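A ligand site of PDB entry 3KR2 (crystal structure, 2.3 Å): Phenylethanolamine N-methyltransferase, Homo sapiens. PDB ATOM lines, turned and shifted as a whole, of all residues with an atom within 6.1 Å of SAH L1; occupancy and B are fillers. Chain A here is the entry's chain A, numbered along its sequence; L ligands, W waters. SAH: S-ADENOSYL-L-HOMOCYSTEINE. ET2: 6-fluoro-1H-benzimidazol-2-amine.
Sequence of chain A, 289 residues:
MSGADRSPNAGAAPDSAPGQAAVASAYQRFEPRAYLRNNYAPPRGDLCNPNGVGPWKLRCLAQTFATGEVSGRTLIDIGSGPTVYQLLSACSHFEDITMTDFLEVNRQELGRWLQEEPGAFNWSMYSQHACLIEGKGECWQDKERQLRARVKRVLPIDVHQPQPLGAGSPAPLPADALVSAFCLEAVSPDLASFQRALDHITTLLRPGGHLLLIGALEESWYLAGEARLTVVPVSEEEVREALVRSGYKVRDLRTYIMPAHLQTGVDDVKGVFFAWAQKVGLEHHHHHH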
ATOM      1  N   TYR A  27      22.493 -19.551   0.494  1.00  0.00           N
ATOM      2  CA  TYR A  27      23.219 -18.960   1.619  1.00  0.00           C
ATOM      3  C   TYR A  27      24.645 -19.497   1.706  1.00  0.00           C
ATOM      4  O   TYR A  27      25.469 -18.981   2.475  1.00  0.00           O
ATOM      5  CB  TYR A  27      22.456 -19.146   2.943  1.00  0.00           C
ATOM      6  CG  TYR A  27      21.461 -18.039   3.180  1.00  0.00           C
ATOM      7  CD1 TYR A  27      20.105 -18.226   2.965  1.00  0.00           C
ATOM      8  CD2 TYR A  27      21.899 -16.774   3.575  1.00  0.00           C
ATOM      9  CE1 TYR A  27      19.198 -17.192   3.172  1.00  0.00           C
ATOM     10  CE2 TYR A  27      21.010 -15.750   3.777  1.00  0.00           C
ATOM     11  CZ  TYR A  27      19.680 -15.949   3.578  1.00  0.00           C
ATOM     12  OH  TYR A  27      18.817 -14.900   3.769  1.00  0.00           O
ATOM     13  N   PHE A  30      26.834 -16.777   0.277  1.00  0.00           N
ATOM     14  CA  PHE A  30      26.723 -15.537   1.054  1.00  0.00           C
ATOM     15  C   PHE A  30      28.070 -14.991   1.563  1.00  0.00           C
ATOM     16  O   PHE A  30      28.707 -15.617   2.405  1.00  0.00           O
ATOM     17  CB  PHE A  30      25.762 -15.818   2.221  1.00  0.00           C
ATOM     18  CG  PHE A  30      25.501 -14.651   3.118  1.00  0.00           C
ATOM     19  CD1 PHE A  30      24.332 -13.934   3.007  1.00  0.00           C
ATOM     20  CD2 PHE A  30      26.401 -14.311   4.127  1.00  0.00           C
ATOM     21  CE1 PHE A  30      24.066 -12.874   3.860  1.00  0.00           C
ATOM     22  CE2 PHE A  30      26.143 -13.254   4.973  1.00  0.00           C
ATOM     23  CZ  PHE A  30      24.972 -12.541   4.845  1.00  0.00           C
ATOM     24  N   TYR A  35      27.990  -8.330   2.290  1.00  0.00           N
ATOM     25  CA  TYR A  35      26.731  -7.988   2.964  1.00  0.00           C
ATOM     26  C   TYR A  35      26.894  -6.711   3.788  1.00  0.00           C
ATOM     27  O   TYR A  35      26.169  -5.745   3.607  1.00  0.00           O
ATOM     28  CB  TYR A  35      26.239  -9.142   3.856  1.00  0.00           C
ATOM     29  CG  TYR A  35      24.994  -8.810   4.658  1.00  0.00           C
ATOM     30  CD1 TYR A  35      23.740  -8.770   4.061  1.00  0.00           C
ATOM     31  CD2 TYR A  35      25.073  -8.541   6.022  1.00  0.00           C
ATOM     32  CE1 TYR A  35      22.602  -8.472   4.795  1.00  0.00           C
ATOM     33  CE2 TYR A  35      23.933  -8.246   6.770  1.00  0.00           C
ATOM     34  CZ  TYR A  35      22.704  -8.210   6.140  1.00  0.00           C
ATOM     35  OH  TYR A  35      21.584  -7.912   6.878  1.00  0.00           O
ATOM     36  N   TYR A  40      25.737  -1.629   5.579  1.00  0.00           N
ATOM     37  CA  TYR A  40      26.249  -0.959   6.776  1.00  0.00           C
ATOM     38  C   TYR A  40      27.458  -0.054   6.512  1.00  0.00           C
ATOM     39  O   TYR A  40      28.138   0.349   7.452  1.00  0.00           O
ATOM     40  CB  TYR A  40      26.537  -1.999   7.867  1.00  0.00           C
ATOM     41  CG  TYR A  40      25.280  -2.771   8.199  1.00  0.00           C
ATOM     42  CD1 TYR A  40      25.069  -4.049   7.708  1.00  0.00           C
ATOM     43  CD2 TYR A  40      24.262  -2.177   8.947  1.00  0.00           C
ATOM     44  CE1 TYR A  40      23.910  -4.744   7.999  1.00  0.00           C
ATOM     45  CE2 TYR A  40      23.097  -2.856   9.241  1.00  0.00           C
ATOM     46  CZ  TYR A  40      22.919  -4.149   8.761  1.00  0.00           C
ATOM     47  OH  TYR A  40      21.765  -4.836   9.026  1.00  0.00           O
ATOM     48  N   LYS A  57      16.588   2.789  12.975  1.00  0.00           N
ATOM     49  CA  LYS A  57      16.694   1.504  13.656  1.00  0.00           C
ATOM     50  C   LYS A  57      17.226   1.646  15.078  1.00  0.00           C
ATOM     51  O   LYS A  57      16.583   1.168  16.038  1.00  0.00           O
ATOM     52  CB  LYS A  57      17.575   0.539  12.856  1.00  0.00           C
ATOM     53  CG  LYS A  57      16.989   0.186  11.510  1.00  0.00           C
ATOM     54  CD  LYS A  57      17.763  -0.927  10.812  1.00  0.00           C
ATOM     55  CE  LYS A  57      19.048  -0.426  10.191  1.00  0.00           C
ATOM     56  NZ  LYS A  57      19.890  -1.561   9.839  1.00  0.00           N
ATOM     57  N   ASP A  77      20.012 -13.398  20.294  1.00  0.00           N
ATOM     58  CA  ASP A  77      19.895 -12.689  19.035  1.00  0.00           C
ATOM     59  C   ASP A  77      19.811 -13.730  17.939  1.00  0.00           C
ATOM     60  O   ASP A  77      20.731 -14.534  17.772  1.00  0.00           O
ATOM     61  CB  ASP A  77      21.099 -11.754  18.801  1.00  0.00           C
ATOM     62  CG  ASP A  77      20.988 -10.977  17.493  1.00  0.00           C
ATOM     63  OD1 ASP A  77      19.864 -10.540  17.177  1.00  0.00           O
ATOM     64  OD2 ASP A  77      22.002 -10.808  16.794  1.00  0.00           O
ATOM     65  N   ILE A  78      18.691 -13.728  17.211  1.00  0.00           N
ATOM     66  CA  ILE A  78      18.397 -14.756  16.215  1.00  0.00           C
ATOM     67  C   ILE A  78      18.889 -14.341  14.847  1.00  0.00           C
ATOM     68  O   ILE A  78      18.400 -13.365  14.278  1.00  0.00           O
ATOM     69  CB  ILE A  78      16.868 -15.002  16.058  1.00  0.00           C
ATOM     70  CG1 ILE A  78      16.193 -15.283  17.406  1.00  0.00           C
ATOM     71  CG2 ILE A  78      16.617 -16.118  15.018  1.00  0.00           C
ATOM     72  CD1 ILE A  78      16.820 -16.421  18.201  1.00  0.00           C
ATOM     73  N   GLY A  79      19.803 -15.124  14.296  1.00  0.00           N
ATOM     74  CA  GLY A  79      20.288 -14.842  12.951  1.00  0.00           C
ATOM     75  C   GLY A  79      21.043 -13.526  12.943  1.00  0.00           C
ATOM     76  O   GLY A  79      20.751 -12.623  12.159  1.00  0.00           O
ATOM     77  N   SER A  80      22.038 -13.440  13.823  1.00  0.00           N
ATOM     78  CA  SER A  80      22.817 -12.239  14.022  1.00  0.00           C
ATOM     79  C   SER A  80      23.513 -11.812  12.753  1.00  0.00           C
ATOM     80  O   SER A  80      23.747 -10.622  12.547  1.00  0.00           O
ATOM     81  CB  SER A  80      23.883 -12.487  15.099  1.00  0.00           C
ATOM     82  OG  SER A  80      23.309 -13.003  16.288  1.00  0.00           O
ATOM     83  N   GLY A  81      23.857 -12.783  11.925  1.00  0.00           N
ATOM     84  CA  GLY A  81      24.733 -12.523  10.794  1.00  0.00           C
ATOM     85  C   GLY A  81      26.101 -12.058  11.279  1.00  0.00           C
ATOM     86  O   GLY A  81      26.585 -12.499  12.330  1.00  0.00           O
ATOM     87  N   PRO A  82      26.745 -11.161  10.510  1.00  0.00           N
ATOM     88  CA  PRO A  82      28.020 -10.563  10.920  1.00  0.00           C
ATOM     89  C   PRO A  82      27.792  -9.211  11.589  1.00  0.00           C
ATOM     90  O   PRO A  82      28.699  -8.385  11.524  1.00  0.00           O
ATOM     91  CB  PRO A  82      28.732 -10.301   9.590  1.00  0.00           C
ATOM     92  CG  PRO A  82      27.628 -10.316   8.533  1.00  0.00           C
ATOM     93  CD  PRO A  82      26.318 -10.641   9.202  1.00  0.00           C
ATOM     94  N   THR A  83      26.611  -8.946  12.164  1.00  0.00           N
ATOM     95  CA  THR A  83      26.361  -7.587  12.666  1.00  0.00           C
ATOM     96  C   THR A  83      26.090  -7.541  14.164  1.00  0.00           C
ATOM     97  O   THR A  83      25.605  -8.504  14.734  1.00  0.00           O
ATOM     98  CB  THR A  83      25.198  -6.868  11.914  1.00  0.00           C
ATOM     99  OG1 THR A  83      23.935  -7.369  12.375  1.00  0.00           O
ATOM    100  CG2 THR A  83      25.325  -7.034  10.390  1.00  0.00           C
ATOM    101  N   TYR A  85      25.025  -4.181  15.698  1.00  0.00           N
ATOM    102  CA  TYR A  85      24.328  -2.927  16.016  1.00  0.00           C
ATOM    103  C   TYR A  85      23.022  -3.218  16.724  1.00  0.00           C
ATOM    104  O   TYR A  85      22.523  -2.386  17.490  1.00  0.00           O
ATOM    105  CB  TYR A  85      24.034  -2.151  14.736  1.00  0.00           C
ATOM    106  CG  TYR A  85      22.957  -2.821  13.924  1.00  0.00           C
ATOM    107  CD1 TYR A  85      21.625  -2.425  14.022  1.00  0.00           C
ATOM    108  CD2 TYR A  85      23.263  -3.884  13.071  1.00  0.00           C
ATOM    109  CE1 TYR A  85      20.637  -3.050  13.294  1.00  0.00           C
ATOM    110  CE2 TYR A  85      22.263  -4.515  12.316  1.00  0.00           C
ATOM    111  CZ  TYR A  85      20.966  -4.105  12.448  1.00  0.00           C
ATOM    112  OH  TYR A  85      19.977  -4.706  11.726  1.00  0.00           O
ATOM    113  N   GLN A  86      22.444  -4.393  16.464  1.00  0.00           N
ATOM    114  CA  GLN A  86      21.128  -4.732  16.994  1.00  0.00           C
ATOM    115  C   GLN A  86      21.152  -5.031  18.497  1.00  0.00           C
ATOM    116  O   GLN A  86      20.102  -5.181  19.118  1.00  0.00           O
ATOM    117  CB  GLN A  86      20.481  -5.884  16.202  1.00  0.00           C
ATOM    118  CG  GLN A  86      21.157  -7.271  16.338  1.00  0.00           C
ATOM    119  CD  GLN A  86      22.271  -7.479  15.331  1.00  0.00           C
ATOM    120  OE1 GLN A  86      22.716  -6.554  14.668  1.00  0.00           O
ATOM    121  NE2 GLN A  86      22.730  -8.719  15.219  1.00  0.00           N
ATOM    122  N   ASP A 101      23.976 -17.631  14.390  1.00  0.00           N
ATOM    123  CA  ASP A 101      23.738 -17.598  12.958  1.00  0.00           C
ATOM    124  C   ASP A 101      23.879 -18.962  12.305  1.00  0.00           C
ATOM    125  O   ASP A 101      24.580 -19.848  12.801  1.00  0.00           O
ATOM    126  CB  ASP A 101      24.615 -16.602  12.214  1.00  0.00           C
ATOM    127  CG  ASP A 101      24.002 -16.200  10.879  1.00  0.00           C
ATOM    128  OD1 ASP A 101      22.912 -15.573  10.888  1.00  0.00           O
ATOM    129  OD2 ASP A 101      24.605 -16.501   9.826  1.00  0.00           O
ATOM    130  N   PHE A 102      23.216 -19.105  11.168  1.00  0.00           N
ATOM    131  CA  PHE A 102      23.210 -20.361  10.436  1.00  0.00           C
ATOM    132  C   PHE A 102      24.565 -20.628   9.794  1.00  0.00           C
ATOM    133  O   PHE A 102      25.017 -21.761   9.746  1.00  0.00           O
ATOM    134  CB  PHE A 102      22.085 -20.332   9.401  1.00  0.00           C
ATOM    135  CG  PHE A 102      21.993 -21.570   8.550  1.00  0.00           C
ATOM    136  CD1 PHE A 102      21.558 -22.772   9.091  1.00  0.00           C
ATOM    137  CD2 PHE A 102      22.302 -21.515   7.213  1.00  0.00           C
ATOM    138  CE1 PHE A 102      21.461 -23.915   8.294  1.00  0.00           C
ATOM    139  CE2 PHE A 102      22.209 -22.641   6.399  1.00  0.00           C
ATOM    140  CZ  PHE A 102      21.791 -23.843   6.943  1.00  0.00           C
ATOM    141  N   LEU A 103      25.234 -19.568   9.335  1.00  0.00           N
ATOM    142  CA  LEU A 103      26.497 -19.735   8.602  1.00  0.00           C
ATOM    143  C   LEU A 103      27.699 -19.673   9.506  1.00  0.00           C
ATOM    144  O   LEU A 103      27.791 -18.817  10.384  1.00  0.00           O
ATOM    145  CB  LEU A 103      26.635 -18.677   7.504  1.00  0.00           C
ATOM    146  CG  LEU A 103      25.596 -18.764   6.390  1.00  0.00           C
ATOM    147  CD1 LEU A 103      25.712 -17.623   5.376  1.00  0.00           C
ATOM    148  CD2 LEU A 103      25.697 -20.149   5.700  1.00  0.00           C
ATOM    149  N   ASN A 106      29.734 -16.268   9.125  1.00  0.00           N
ATOM    150  CA  ASN A 106      29.247 -15.135   9.920  1.00  0.00           C
ATOM    151  C   ASN A 106      29.639 -15.254  11.370  1.00  0.00           C
ATOM    152  O   ASN A 106      29.993 -14.257  11.998  1.00  0.00           O
ATOM    153  CB  ASN A 106      27.727 -15.018   9.830  1.00  0.00           C
ATOM    154  CG  ASN A 106      27.276 -14.406   8.525  1.00  0.00           C
ATOM    155  OD1 ASN A 106      26.164 -14.690   8.045  1.00  0.00           O
ATOM    156  ND2 ASN A 106      28.122 -13.570   7.941  1.00  0.00           N
ATOM    157  N   ILE A 157      22.457 -21.920  14.413  1.00  0.00           N
ATOM    158  CA  ILE A 157      21.009 -21.973  14.586  1.00  0.00           C
ATOM    159  C   ILE A 157      20.352 -22.179  13.217  1.00  0.00           C
ATOM    160  O   ILE A 157      20.931 -21.772  12.194  1.00  0.00           O
ATOM    161  CB  ILE A 157      20.522 -20.647  15.222  1.00  0.00           C
ATOM    162  CG1 ILE A 157      19.041 -20.736  15.601  1.00  0.00           C
ATOM    163  CG2 ILE A 157      20.765 -19.482  14.279  1.00  0.00           C
ATOM    164  CD1 ILE A 157      18.527 -19.508  16.333  1.00  0.00           C
ATOM    165  N   ASP A 158      19.193 -22.839  13.205  1.00  0.00           N
ATOM    166  CA  ASP A 158      18.329 -22.975  12.011  1.00  0.00           C
ATOM    167  C   ASP A 158      16.872 -22.781  12.410  1.00  0.00           C
ATOM    168  O   ASP A 158      16.271 -23.647  13.062  1.00  0.00           O
ATOM    169  CB  ASP A 158      18.463 -24.372  11.392  1.00  0.00           C
ATOM    170  CG  ASP A 158      17.658 -24.528  10.086  1.00  0.00           C
ATOM    171  OD1 ASP A 158      16.766 -23.683   9.792  1.00  0.00           O
ATOM    172  OD2 ASP A 158      17.908 -25.493   9.337  1.00  0.00           O
ATOM    173  N   VAL A 159      16.298 -21.660  12.003  1.00  0.00           N
ATOM    174  CA  VAL A 159      14.933 -21.344  12.416  1.00  0.00           C
ATOM    175  C   VAL A 159      13.892 -22.286  11.803  1.00  0.00           C
ATOM    176  O   VAL A 159      12.730 -22.310  12.239  1.00  0.00           O
ATOM    177  CB  VAL A 159      14.562 -19.888  12.103  1.00  0.00           C
ATOM    178  CG1 VAL A 159      15.308 -18.958  13.053  1.00  0.00           C
ATOM    179  CG2 VAL A 159      14.915 -19.579  10.663  1.00  0.00           C
ATOM    180  N   HIS A 160      14.307 -23.053  10.797  1.00  0.00           N
ATOM    181  CA  HIS A 160      13.425 -24.015  10.153  1.00  0.00           C
ATOM    182  C   HIS A 160      13.196 -25.237  11.054  1.00  0.00           C
ATOM    183  O   HIS A 160      12.248 -25.988  10.847  1.00  0.00           O
ATOM    184  CB  HIS A 160      13.989 -24.424   8.803  1.00  0.00           C
ATOM    185  CG  HIS A 160      14.096 -23.293   7.829  1.00  0.00           C
ATOM    186  ND1 HIS A 160      13.109 -22.327   7.710  1.00  0.00           N
ATOM    187  CD2 HIS A 160      15.059 -22.960   6.937  1.00  0.00           C
ATOM    188  CE1 HIS A 160      13.468 -21.452   6.784  1.00  0.00           C
ATOM    189  NE2 HIS A 160      14.640 -21.824   6.299  1.00  0.00           N
ATOM    190  N   SER A 180      15.713 -10.185  16.682  1.00  0.00           N
ATOM    191  CA  SER A 180      16.035 -10.680  15.354  1.00  0.00           C
ATOM    192  C   SER A 180      15.818  -9.609  14.317  1.00  0.00           C
ATOM    193  O   SER A 180      14.731  -9.033  14.224  1.00  0.00           O
ATOM    194  CB  SER A 180      15.203 -11.903  14.982  1.00  0.00           C
ATOM    195  OG  SER A 180      15.623 -12.416  13.722  1.00  0.00           O
ATOM    196  N   ALA A 181      16.857  -9.371  13.529  1.00  0.00           N
ATOM    197  CA  ALA A 181      16.783  -8.379  12.480  1.00  0.00           C
ATOM    198  C   ALA A 181      17.107  -8.960  11.107  1.00  0.00           C
ATOM    199  O   ALA A 181      18.145  -9.584  10.930  1.00  0.00           O
ATOM    200  CB  ALA A 181      17.712  -7.205  12.808  1.00  0.00           C
ATOM    201  N   PHE A 182      16.197  -8.755  10.156  1.00  0.00           N
ATOM    202  CA  PHE A 182      16.438  -9.134   8.773  1.00  0.00           C
ATOM    203  C   PHE A 182      16.690 -10.627   8.536  1.00  0.00           C
ATOM    204  O   PHE A 182      17.382 -11.018   7.583  1.00  0.00           O
ATOM    205  CB  PHE A 182      17.573  -8.289   8.217  1.00  0.00           C
ATOM    206  CG  PHE A 182      17.269  -6.822   8.205  1.00  0.00           C
ATOM    207  CD1 PHE A 182      17.924  -5.951   9.074  1.00  0.00           C
ATOM    208  CD2 PHE A 182      16.307  -6.315   7.352  1.00  0.00           C
ATOM    209  CE1 PHE A 182      17.633  -4.601   9.072  1.00  0.00           C
ATOM    210  CE2 PHE A 182      16.008  -4.962   7.356  1.00  0.00           C
ATOM    211  CZ  PHE A 182      16.677  -4.109   8.216  1.00  0.00           C
ATOM    212  N   CYS A 183      16.113 -11.473   9.377  1.00  0.00           N
ATOM    213  CA  CYS A 183      16.311 -12.901   9.257  1.00  0.00           C
ATOM    214  C   CYS A 183      15.116 -13.644   8.632  1.00  0.00           C
ATOM    215  O   CYS A 183      15.172 -14.079   7.478  1.00  0.00           O
ATOM    216  CB  CYS A 183      16.663 -13.491  10.613  1.00  0.00           C
ATOM    217  SG  CYS A 183      17.055 -15.256  10.552  1.00  0.00           S
ATOM    218  N   ALA A 186      13.930 -13.249   5.304  1.00  0.00           N
ATOM    219  CA  ALA A 186      15.054 -13.500   4.415  1.00  0.00           C
ATOM    220  C   ALA A 186      15.427 -14.985   4.296  1.00  0.00           C
ATOM    221  O   ALA A 186      16.296 -15.327   3.492  1.00  0.00           O
ATOM    222  CB  ALA A 186      16.259 -12.713   4.882  1.00  0.00           C
ATOM    223  N   VAL A 187      14.819 -15.855   5.094  1.00  0.00           N
ATOM    224  CA  VAL A 187      15.106 -17.290   4.999  1.00  0.00           C
ATOM    225  C   VAL A 187      13.817 -18.063   4.727  1.00  0.00           C
ATOM    226  O   VAL A 187      13.766 -19.281   4.824  1.00  0.00           O
ATOM    227  CB  VAL A 187      15.801 -17.849   6.266  1.00  0.00           C
ATOM    228  CG1 VAL A 187      17.010 -17.014   6.611  1.00  0.00           C
ATOM    229  CG2 VAL A 187      14.836 -17.876   7.446  1.00  0.00           C
ATOM    230  N   TYR A 222      17.836  -9.796  -2.229  1.00  0.00           N
ATOM    231  CA  TYR A 222      18.993  -8.973  -1.890  1.00  0.00           C
ATOM    232  C   TYR A 222      20.258  -9.761  -2.202  1.00  0.00           C
ATOM    233  O   TYR A 222      20.248 -10.999  -2.221  1.00  0.00           O
ATOM    234  CB  TYR A 222      18.957  -8.495  -0.437  1.00  0.00           C
ATOM    235  CG  TYR A 222      19.319  -9.544   0.585  1.00  0.00           C
ATOM    236  CD1 TYR A 222      20.600  -9.598   1.110  1.00  0.00           C
ATOM    237  CD2 TYR A 222      18.390 -10.495   1.024  1.00  0.00           C
ATOM    238  CE1 TYR A 222      20.959 -10.546   2.046  1.00  0.00           C
ATOM    239  CE2 TYR A 222      18.745 -11.459   1.977  1.00  0.00           C
ATOM    240  CZ  TYR A 222      20.032 -11.469   2.478  1.00  0.00           C
ATOM    241  OH  TYR A 222      20.416 -12.392   3.403  1.00  0.00           O
HETATM  242  N   SAH L   1      20.766  -9.738  11.585  1.00  0.00           N
HETATM  243  CA  SAH L   1      21.780  -9.220  10.686  1.00  0.00           C
HETATM  244  CB  SAH L   1      21.951 -10.148   9.481  1.00  0.00           C
HETATM  245  CG  SAH L   1      20.622 -10.480   8.792  1.00  0.00           C
HETATM  246  SD  SAH L   1      20.873 -11.204   7.142  1.00  0.00           S
HETATM  247  C   SAH L   1      21.376  -7.818  10.247  1.00  0.00           C
HETATM  248  O   SAH L   1      22.009  -7.312   9.389  1.00  0.00           O
HETATM  249  OXT SAH L   1      20.361  -7.221  10.982  1.00  0.00           O
HETATM  250  C5' SAH L   1      20.025 -12.805   7.347  1.00  0.00           C
HETATM  251  C4' SAH L   1      20.801 -13.827   8.175  1.00  0.00           C
HETATM  252  O4' SAH L   1      20.010 -14.958   8.231  1.00  0.00           O
HETATM  253  C3' SAH L   1      22.064 -14.278   7.450  1.00  0.00           C
HETATM  254  O3' SAH L   1      23.180 -13.997   8.273  1.00  0.00           O
HETATM  255  C2' SAH L   1      21.864 -15.637   7.262  1.00  0.00           C
HETATM  256  O2' SAH L   1      23.014 -16.433   7.348  1.00  0.00           O
HETATM  257  C1' SAH L   1      20.912 -16.013   8.241  1.00  0.00           C
HETATM  258  N9  SAH L   1      20.288 -17.305   7.971  1.00  0.00           N
HETATM  259  C8  SAH L   1      20.242 -17.925   6.784  1.00  0.00           C
HETATM  260  N7  SAH L   1      19.541 -19.095   6.939  1.00  0.00           N
HETATM  261  C5  SAH L   1      19.144 -19.190   8.239  1.00  0.00           C
HETATM  262  C6  SAH L   1      18.430 -20.142   8.919  1.00  0.00           C
HETATM  263  N6  SAH L   1      17.927 -21.307   8.200  1.00  0.00           N
HETATM  264  N1  SAH L   1      18.170 -19.993  10.208  1.00  0.00           N
HETATM  265  C2  SAH L   1      18.621 -18.894  10.861  1.00  0.00           C
HETATM  266  N3  SAH L   1      19.339 -17.960  10.192  1.00  0.00           N
HETATM  267  C4  SAH L   1      19.585 -18.106   8.886  1.00  0.00           C
HETATM  268  NAA ET2 L   2      19.395  -6.889   5.752  1.00  0.00           N
HETATM  269  FAB ET2 L   2      18.104  -0.069   4.360  1.00  0.00           F
HETATM  270  CAC ET2 L   2      19.596  -1.081   5.906  1.00  0.00           C
HETATM  271  CAD ET2 L   2      20.142  -2.223   6.473  1.00  0.00           C
HETATM  272  CAE ET2 L   2      18.211  -2.444   4.488  1.00  0.00           C
HETATM  273  NAF ET2 L   2      18.555  -4.874   4.855  1.00  0.00           N
HETATM  274  NAG ET2 L   2      20.069  -4.703   6.408  1.00  0.00           N
HETATM  275  CAH ET2 L   2      18.630  -1.191   4.913  1.00  0.00           C
HETATM  276  CAI ET2 L   2      19.349  -5.562   5.677  1.00  0.00           C
HETATM  277  CAJ ET2 L   2      18.762  -3.578   5.059  1.00  0.00           C
HETATM  278  CAK ET2 L   2      19.728  -3.468   6.051  1.00  0.00           C
HETATM  279  O   HOH W   1      19.628 -10.460  14.406  1.00  0.00           O
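OH of Tyr 40 is in hydrogen-bond range of O of SAH L1.
OH of Tyr 35 is in hydrogen-bond range of O of SAH L1, at 2.6 Å.
OH of Tyr 85 is in hydrogen-bond range of OXT of SAH L1 (2.7 Å).
O of Ala 181 sits at hydrogen-bond distance from N of SAH L1 (2.7 Å).
O of Gly 79 lies within hydrogen-bond range of N of SAH L1 (2.9 Å).
An oxygen (O2') of SAH L1 is in hydrogen-bond range of the side-chain carboxylate (OD2) of Asp 101, 2.9 Å away.
A nitrogen (N) of SAH L1 sits close to the backbone carbonyl oxygen of Ser 80 (3.3 Å).
O3' of SAH L1 is in hydrogen-bond range of OD1 of Asn 106 (3.1 Å).
The backbone NH (N) of Val 159 sits at hydrogen-bond distance from a nitrogen (N1) of SAH L1 (3.1 Å).
The side-chain carboxylate of Asp 158 lies within hydrogen-bond range of a nitrogen (N6) of SAH L1 (3.1 Å).
The side-chain sulfur (SG) of Cys 183 is in hydrogen-bond range of a nitrogen (N3) of SAH L1 (3.6 Å).
OH of Tyr 40 sits at hydrogen-bond distance from NAG of ET2 L2, at 3.1 Å.
NAA of ET2 L2 is in hydrogen-bond range of OH of Tyr 35.
OD2 of Asp 101 sits close to OD1 of Asn 106.
The backbone NH (N) of Leu 103 sits at hydrogen-bond distance from the side-chain carboxylate (OD2) of Asp 101.
O of Asp 101 sits at hydrogen-bond distance from N of Ile 157, 3.4 Å away.
NE2 of Gln 86 is in hydrogen-bond range of O of Ser 80, 3.4 Å away.
The side-chain hydroxyl (OG) of Ser 80 sits at hydrogen-bond distance from the side-chain carboxylate (OD2) of Asp 77 (2.6 Å).
OD1 of Asp 158 is in hydrogen-bond range of N of His 160 (2.7 Å).
O of Val 187 sits close to NE2 of His 160, 3.1 Å away.
The side-chain hydroxyl of Tyr 222 lies within hydrogen-bond range of the side-chain hydroxyl of Tyr 27 (3.0 Å).
The backbone carbonyl oxygen (O) of Phe 182 sits close to a sulfur (SD) of SAH L1 (3.5 Å).
Tyr 27 touches SAH L1 (CE2 to C2', 3.6 Å).
CA of Gly 81 touches O3' of SAH L1 (3.3 Å).
OG1 of Thr 83 touches CA of SAH L1 (3.3 Å).
CB of Phe 102 touches C5 of SAH L1, at 3.4 Å.
CD1 of Leu 103 touches O2' of SAH L1, 3.5 Å away.
Ile 157 touches SAH L1.
His 160 touches SAH L1.
CG1 of Val 187 touches N7 of SAH L1, at 3.3 Å.
Tyr 222 touches SAH L1.
Within 4 Å of SAH L1: Tyr 27, Tyr 35, Tyr 40, Gly 79, Ser 80, Gly 81, Thr 83, Tyr 85, Asp 101, Phe 102, Leu 103, Asn 106, Ile 157, Asp 158, Val 159, His 160, Ala 181, Phe 182, Cys 183, Val 187 and Tyr 222.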
